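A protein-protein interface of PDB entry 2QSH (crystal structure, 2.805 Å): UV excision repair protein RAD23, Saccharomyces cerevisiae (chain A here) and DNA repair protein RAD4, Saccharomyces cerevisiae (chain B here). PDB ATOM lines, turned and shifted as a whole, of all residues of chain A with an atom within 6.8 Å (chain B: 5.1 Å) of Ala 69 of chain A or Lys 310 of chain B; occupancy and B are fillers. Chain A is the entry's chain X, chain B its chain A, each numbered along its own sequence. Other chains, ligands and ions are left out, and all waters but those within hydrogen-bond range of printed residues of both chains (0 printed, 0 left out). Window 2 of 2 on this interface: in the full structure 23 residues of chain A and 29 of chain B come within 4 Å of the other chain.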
ATOM      1  N   ARG A  64     -11.644 -25.709 -17.435  1.00  0.00           N
ATOM      2  CA  ARG A  64     -10.407 -24.971 -17.648  1.00  0.00           C
ATOM      3  C   ARG A  64     -10.488 -23.584 -17.019  1.00  0.00           C
ATOM      4  O   ARG A  64      -9.669 -23.231 -16.167  1.00  0.00           O
ATOM      5  CB  ARG A  64     -10.089 -24.896 -19.147  1.00  0.00           C
ATOM      6  CG  ARG A  64      -9.346 -23.640 -19.617  1.00  0.00           C
ATOM      7  CD  ARG A  64      -7.851 -23.802 -19.541  1.00  0.00           C
ATOM      8  NE  ARG A  64      -7.302 -24.521 -20.692  1.00  0.00           N
ATOM      9  CZ  ARG A  64      -6.631 -23.944 -21.686  1.00  0.00           C
ATOM     10  NH1 ARG A  64      -6.426 -22.631 -21.675  1.00  0.00           N
ATOM     11  NH2 ARG A  64      -6.159 -24.680 -22.688  1.00  0.00           N
ATOM     12  N   GLU A  65     -11.500 -22.820 -17.413  1.00  0.00           N
ATOM     13  CA  GLU A  65     -11.623 -21.440 -16.974  1.00  0.00           C
ATOM     14  C   GLU A  65     -11.982 -21.355 -15.494  1.00  0.00           C
ATOM     15  O   GLU A  65     -11.652 -20.373 -14.819  1.00  0.00           O
ATOM     16  CB  GLU A  65     -12.632 -20.681 -17.850  1.00  0.00           C
ATOM     17  CG  GLU A  65     -12.407 -19.162 -17.901  1.00  0.00           C
ATOM     18  CD  GLU A  65     -10.928 -18.776 -17.822  1.00  0.00           C
ATOM     19  OE1 GLU A  65     -10.142 -19.179 -18.715  1.00  0.00           O
ATOM     20  OE2 GLU A  65     -10.554 -18.075 -16.854  1.00  0.00           O
ATOM     21  N   HIS A  66     -12.638 -22.401 -14.998  1.00  0.00           N
ATOM     22  CA  HIS A  66     -13.072 -22.454 -13.613  1.00  0.00           C
ATOM     23  C   HIS A  66     -11.889 -22.612 -12.680  1.00  0.00           C
ATOM     24  O   HIS A  66     -11.747 -21.850 -11.727  1.00  0.00           O
ATOM     25  CB  HIS A  66     -14.066 -23.595 -13.403  1.00  0.00           C
ATOM     26  CG  HIS A  66     -14.720 -23.582 -12.056  1.00  0.00           C
ATOM     27  ND1 HIS A  66     -14.697 -24.668 -11.206  1.00  0.00           N
ATOM     28  CD2 HIS A  66     -15.411 -22.613 -11.408  1.00  0.00           C
ATOM     29  CE1 HIS A  66     -15.350 -24.372 -10.096  1.00  0.00           C
ATOM     30  NE2 HIS A  66     -15.790 -23.129 -10.192  1.00  0.00           N
ATOM     31  N   ILE A  67     -11.046 -23.603 -12.971  1.00  0.00           N
ATOM     32  CA  ILE A  67      -9.863 -23.916 -12.169  1.00  0.00           C
ATOM     33  C   ILE A  67      -8.930 -22.715 -12.067  1.00  0.00           C
ATOM     34  O   ILE A  67      -8.429 -22.392 -10.986  1.00  0.00           O
ATOM     35  CB  ILE A  67      -9.084 -25.115 -12.773  1.00  0.00           C
ATOM     36  CG1 ILE A  67      -9.925 -26.394 -12.723  1.00  0.00           C
ATOM     37  CG2 ILE A  67      -7.746 -25.326 -12.070  1.00  0.00           C
ATOM     38  CD1 ILE A  67     -10.033 -27.032 -11.357  1.00  0.00           C
ATOM     39  N   MET A  68      -8.719 -22.058 -13.202  1.00  0.00           N
ATOM     40  CA  MET A  68      -7.788 -20.951 -13.303  1.00  0.00           C
ATOM     41  C   MET A  68      -8.179 -19.768 -12.406  1.00  0.00           C
ATOM     42  O   MET A  68      -7.323 -19.161 -11.758  1.00  0.00           O
ATOM     43  CB  MET A  68      -7.681 -20.503 -14.759  1.00  0.00           C
ATOM     44  CG  MET A  68      -6.255 -20.340 -15.231  1.00  0.00           C
ATOM     45  SD  MET A  68      -5.608 -21.810 -16.050  1.00  0.00           S
ATOM     46  CE  MET A  68      -5.882 -21.350 -17.767  1.00  0.00           C
ATOM     47  N   ALA A  69      -9.471 -19.456 -12.363  1.00  0.00           N
ATOM     48  CA  ALA A  69      -9.957 -18.302 -11.607  1.00  0.00           C
ATOM     49  C   ALA A  69     -10.459 -18.655 -10.205  1.00  0.00           C
ATOM     50  O   ALA A  69     -10.333 -17.855  -9.275  1.00  0.00           O
ATOM     51  CB  ALA A  69     -11.036 -17.582 -12.387  1.00  0.00           C
ATOM     52  N   ASN A  70     -11.030 -19.849 -10.058  1.00  0.00           N
ATOM     53  CA  ASN A  70     -11.640 -20.267  -8.799  1.00  0.00           C
ATOM     54  C   ASN A  70     -11.185 -21.651  -8.337  1.00  0.00           C
ATOM     55  O   ASN A  70     -11.988 -22.581  -8.296  1.00  0.00           O
ATOM     56  CB  ASN A  70     -13.168 -20.263  -8.921  1.00  0.00           C
ATOM     57  CG  ASN A  70     -13.731 -18.911  -9.298  1.00  0.00           C
ATOM     58  OD1 ASN A  70     -13.215 -17.872  -8.891  1.00  0.00           O
ATOM     59  ND2 ASN A  70     -14.810 -18.920 -10.075  1.00  0.00           N
ATOM     60  N   PRO A  71      -9.908 -21.793  -7.958  1.00  0.00           N
ATOM     61  CA  PRO A  71      -9.456 -23.128  -7.580  1.00  0.00           C
ATOM     62  C   PRO A  71     -10.058 -23.611  -6.254  1.00  0.00           C
ATOM     63  O   PRO A  71     -10.240 -24.815  -6.076  1.00  0.00           O
ATOM     64  CB  PRO A  71      -7.931 -22.979  -7.452  1.00  0.00           C
ATOM     65  CG  PRO A  71      -7.602 -21.577  -7.808  1.00  0.00           C
ATOM     66  CD  PRO A  71      -8.850 -20.777  -7.825  1.00  0.00           C
ATOM     67  N   GLU A  72     -10.362 -22.678  -5.348  1.00  0.00           N
ATOM     68  CA  GLU A  72     -10.886 -23.009  -4.017  1.00  0.00           C
ATOM     69  C   GLU A  72     -12.261 -23.642  -4.118  1.00  0.00           C
ATOM     70  O   GLU A  72     -12.586 -24.565  -3.365  1.00  0.00           O
ATOM     71  CB  GLU A  72     -11.007 -21.775  -3.109  1.00  0.00           C
ATOM     72  CG  GLU A  72     -10.182 -20.556  -3.489  1.00  0.00           C
ATOM     73  CD  GLU A  72     -10.882 -19.666  -4.509  1.00  0.00           C
ATOM     74  OE1 GLU A  72     -11.042 -20.109  -5.666  1.00  0.00           O
ATOM     75  OE2 GLU A  72     -11.254 -18.523  -4.160  1.00  0.00           O
ATOM     76  N   VAL A  73     -13.068 -23.119  -5.038  1.00  0.00           N
ATOM     77  CA  VAL A  73     -14.408 -23.635  -5.282  1.00  0.00           C
ATOM     78  C   VAL A  73     -14.298 -25.098  -5.671  1.00  0.00           C
ATOM     79  O   VAL A  73     -14.992 -25.951  -5.116  1.00  0.00           O
ATOM     80  CB  VAL A  73     -15.148 -22.849  -6.394  1.00  0.00           C
ATOM     81  CG1 VAL A  73     -16.592 -23.339  -6.531  1.00  0.00           C
ATOM     82  CG2 VAL A  73     -15.117 -21.353  -6.104  1.00  0.00           C
ATOM     83  N   VAL A  75     -11.845 -27.122  -5.055  1.00  0.00           N
ATOM     84  CA  VAL A  75     -11.338 -27.856  -3.895  1.00  0.00           C
ATOM     85  C   VAL A  75     -12.477 -28.307  -2.980  1.00  0.00           C
ATOM     86  O   VAL A  75     -12.624 -29.506  -2.713  1.00  0.00           O
ATOM     87  CB  VAL A  75     -10.291 -27.025  -3.102  1.00  0.00           C
ATOM     88  CG1 VAL A  75      -9.986 -27.673  -1.754  1.00  0.00           C
ATOM     89  CG2 VAL A  75      -9.023 -26.864  -3.910  1.00  0.00           C
ATOM     90  N   PHE B 303       0.344 -14.183 -11.266  1.00  0.00           N
ATOM     91  CA  PHE B 303      -0.928 -14.901 -11.315  1.00  0.00           C
ATOM     92  C   PHE B 303      -0.857 -16.252 -10.598  1.00  0.00           C
ATOM     93  O   PHE B 303      -1.697 -16.555  -9.747  1.00  0.00           O
ATOM     94  CB  PHE B 303      -1.362 -15.097 -12.770  1.00  0.00           C
ATOM     95  CG  PHE B 303      -2.652 -15.848 -12.925  1.00  0.00           C
ATOM     96  CD1 PHE B 303      -3.867 -15.167 -12.956  1.00  0.00           C
ATOM     97  CD2 PHE B 303      -2.656 -17.238 -13.042  1.00  0.00           C
ATOM     98  CE1 PHE B 303      -5.074 -15.857 -13.098  1.00  0.00           C
ATOM     99  CE2 PHE B 303      -3.852 -17.941 -13.180  1.00  0.00           C
ATOM    100  CZ  PHE B 303      -5.067 -17.246 -13.210  1.00  0.00           C
ATOM    101  N   LYS B 306      -0.705 -16.048  -6.718  1.00  0.00           N
ATOM    102  CA  LYS B 306      -2.021 -15.864  -6.117  1.00  0.00           C
ATOM    103  C   LYS B 306      -2.820 -17.156  -6.221  1.00  0.00           C
ATOM    104  O   LYS B 306      -3.503 -17.549  -5.274  1.00  0.00           O
ATOM    105  CB  LYS B 306      -2.787 -14.736  -6.818  1.00  0.00           C
ATOM    106  CG  LYS B 306      -2.071 -13.381  -6.904  1.00  0.00           C
ATOM    107  CD  LYS B 306      -2.488 -12.436  -5.776  1.00  0.00           C
ATOM    108  CE  LYS B 306      -2.610 -10.981  -6.254  1.00  0.00           C
ATOM    109  NZ  LYS B 306      -1.328 -10.430  -6.784  1.00  0.00           N
ATOM    110  N   TRP B 307      -2.717 -17.813  -7.376  1.00  0.00           N
ATOM    111  CA  TRP B 307      -3.435 -19.055  -7.634  1.00  0.00           C
ATOM    112  C   TRP B 307      -3.054 -20.148  -6.651  1.00  0.00           C
ATOM    113  O   TRP B 307      -3.916 -20.881  -6.165  1.00  0.00           O
ATOM    114  CB  TRP B 307      -3.172 -19.541  -9.057  1.00  0.00           C
ATOM    115  CG  TRP B 307      -3.930 -20.780  -9.400  1.00  0.00           C
ATOM    116  CD1 TRP B 307      -5.189 -20.850  -9.912  1.00  0.00           C
ATOM    117  CD2 TRP B 307      -3.482 -22.132  -9.248  1.00  0.00           C
ATOM    118  NE1 TRP B 307      -5.558 -22.159 -10.094  1.00  0.00           N
ATOM    119  CE2 TRP B 307      -4.529 -22.970  -9.693  1.00  0.00           C
ATOM    120  CE3 TRP B 307      -2.296 -22.719  -8.781  1.00  0.00           C
ATOM    121  CZ2 TRP B 307      -4.431 -24.369  -9.685  1.00  0.00           C
ATOM    122  CZ3 TRP B 307      -2.193 -24.116  -8.776  1.00  0.00           C
ATOM    123  CH2 TRP B 307      -3.261 -24.921  -9.221  1.00  0.00           C
ATOM    124  N   PHE B 308      -1.761 -20.265  -6.370  1.00  0.00           N
ATOM    125  CA  PHE B 308      -1.277 -21.316  -5.483  1.00  0.00           C
ATOM    126  C   PHE B 308      -1.683 -21.027  -4.051  1.00  0.00           C
ATOM    127  O   PHE B 308      -1.999 -21.945  -3.291  1.00  0.00           O
ATOM    128  CB  PHE B 308       0.238 -21.445  -5.580  1.00  0.00           C
ATOM    129  CG  PHE B 308       0.792 -22.635  -4.860  1.00  0.00           C
ATOM    130  CD1 PHE B 308       0.540 -23.929  -5.322  1.00  0.00           C
ATOM    131  CD2 PHE B 308       1.586 -22.469  -3.728  1.00  0.00           C
ATOM    132  CE1 PHE B 308       1.070 -25.043  -4.653  1.00  0.00           C
ATOM    133  CE2 PHE B 308       2.129 -23.578  -3.061  1.00  0.00           C
ATOM    134  CZ  PHE B 308       1.869 -24.860  -3.526  1.00  0.00           C
ATOM    135  N   ARG B 309      -1.680 -19.744  -3.698  1.00  0.00           N
ATOM    136  CA  ARG B 309      -2.049 -19.320  -2.364  1.00  0.00           C
ATOM    137  C   ARG B 309      -3.502 -19.701  -2.109  1.00  0.00           C
ATOM    138  O   ARG B 309      -3.884 -20.059  -0.992  1.00  0.00           O
ATOM    139  CB  ARG B 309      -1.849 -17.811  -2.211  1.00  0.00           C
ATOM    140  CG  ARG B 309      -1.119 -17.416  -0.938  1.00  0.00           C
ATOM    141  CD  ARG B 309       0.414 -17.438  -1.128  1.00  0.00           C
ATOM    142  NE  ARG B 309       0.946 -16.104  -1.459  1.00  0.00           N
ATOM    143  CZ  ARG B 309       2.240 -15.801  -1.608  1.00  0.00           C
ATOM    144  NH1 ARG B 309       3.186 -16.732  -1.470  1.00  0.00           N
ATOM    145  NH2 ARG B 309       2.589 -14.551  -1.902  1.00  0.00           N
ATOM    146  N   LYS B 310      -4.303 -19.644  -3.168  1.00  0.00           N
ATOM    147  CA  LYS B 310      -5.708 -19.994  -3.074  1.00  0.00           C
ATOM    148  C   LYS B 310      -5.903 -21.474  -2.771  1.00  0.00           C
ATOM    149  O   LYS B 310      -6.785 -21.830  -1.991  1.00  0.00           O
ATOM    150  CB  LYS B 310      -6.450 -19.624  -4.352  1.00  0.00           C
ATOM    151  CG  LYS B 310      -6.630 -18.148  -4.574  1.00  0.00           C
ATOM    152  CD  LYS B 310      -7.629 -17.934  -5.690  1.00  0.00           C
ATOM    153  CE  LYS B 310      -7.451 -16.595  -6.357  1.00  0.00           C
ATOM    154  NZ  LYS B 310      -8.275 -16.551  -7.587  1.00  0.00           N
ATOM    155  N   VAL B 311      -5.095 -22.332  -3.390  1.00  0.00           N
ATOM    156  CA  VAL B 311      -5.199 -23.770  -3.159  1.00  0.00           C
ATOM    157  C   VAL B 311      -4.812 -24.088  -1.716  1.00  0.00           C
ATOM    158  O   VAL B 311      -5.572 -24.741  -0.991  1.00  0.00           O
ATOM    159  CB  VAL B 311      -4.317 -24.577  -4.128  1.00  0.00           C
ATOM    160  CG1 VAL B 311      -4.528 -26.055  -3.920  1.00  0.00           C
ATOM    161  CG2 VAL B 311      -4.626 -24.205  -5.571  1.00  0.00           C
ATOM    162  N   ILE B 312      -3.640 -23.607  -1.299  1.00  0.00           N
ATOM    163  CA  ILE B 312      -3.179 -23.773   0.073  1.00  0.00           C
ATOM    164  C   ILE B 312      -4.256 -23.359   1.091  1.00  0.00           C
ATOM    165  O   ILE B 312      -4.642 -24.159   1.948  1.00  0.00           O
ATOM    166  CB  ILE B 312      -1.869 -23.002   0.334  1.00  0.00           C
ATOM    167  CG1 ILE B 312      -0.725 -23.555  -0.533  1.00  0.00           C
ATOM    168  CG2 ILE B 312      -1.511 -23.042   1.814  1.00  0.00           C
ATOM    169  CD1 ILE B 312       0.052 -24.735   0.061  1.00  0.00           C
ATOM    170  N   THR B 313      -4.749 -22.125   0.990  1.00  0.00           N
ATOM    171  CA  THR B 313      -5.735 -21.627   1.948  1.00  0.00           C
ATOM    172  C   THR B 313      -6.910 -22.600   2.042  1.00  0.00           C
ATOM    173  O   THR B 313      -7.408 -22.881   3.133  1.00  0.00           O
ATOM    174  CB  THR B 313      -6.244 -20.210   1.587  1.00  0.00           C
ATOM    175  OG1 THR B 313      -5.129 -19.338   1.350  1.00  0.00           O
ATOM    176  CG2 THR B 313      -7.079 -19.642   2.714  1.00  0.00           C
ATOM    177  N   ALA B 314      -7.314 -23.132   0.889  1.00  0.00           N
ATOM    178  CA  ALA B 314      -8.448 -24.045   0.793  1.00  0.00           C
ATOM    179  C   ALA B 314      -8.219 -25.371   1.529  1.00  0.00           C
ATOM    180  O   ALA B 314      -9.183 -26.014   1.945  1.00  0.00           O
ATOM    181  CB  ALA B 314      -8.801 -24.291  -0.667  1.00  0.00           C
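Printed residues of chain A that touch a printed residue of chain B: Ile 67, Met 68, Ala 69, Pro 71, Glu 72 and Val 75.
Hydrophobic or aromatic side chains of chain A that line the printed part of chain B: Met 68, Pro 71 and Val 75.
Of the 10 printed residues of chain B, 5 touch a printed residue of chain A.
Among the printed residues, 9 pairs touch across the chains.
Among the printed residues, no Asp or Glu carboxylate lies within 4 Å of a Lys or Arg side-chain nitrogen of the other chain.
Met 68 of chain A touches Phe 303 of chain B.
CD1 of Trp 307 of chain B touches O of Met 68 of chain A, at 3.3 Å.
CG of Pro 71 of chain A touches NE1 of Trp 307 of chain B, at 3.1 Å.
Lys 310 of chain B touches Pro 71 of chain A.
CB of Pro 71 of chain A touches CG2 of Val 311 of chain B, 3.996 Å away.
Glu 72 of chain A touches Lys 310 of chain B.
CG1 of Val 75 of chain A touches CB of Ala 314 of chain B (3.7 Å).
Printed residues of chain A within 4 Å of Phe 303 of chain B: Met 68.
Of the printed residues of chain A, Trp 307 of chain B touches Ile 67, Met 68 and Pro 71.
Printed residues of chain B within 4 Å of Met 68 of chain A: Phe 303 and Trp 307.
Thr 313 of chain B touches none of the printed residues of chain A.
O of Ile 67 of chain A is in hydrogen-bond range of NE1 of Trp 307 of chain B, 3.0 Å away.
O of Ala 69 of chain A lies within hydrogen-bond range of NZ of Lys 310 of chain B, at 3.0 Å.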
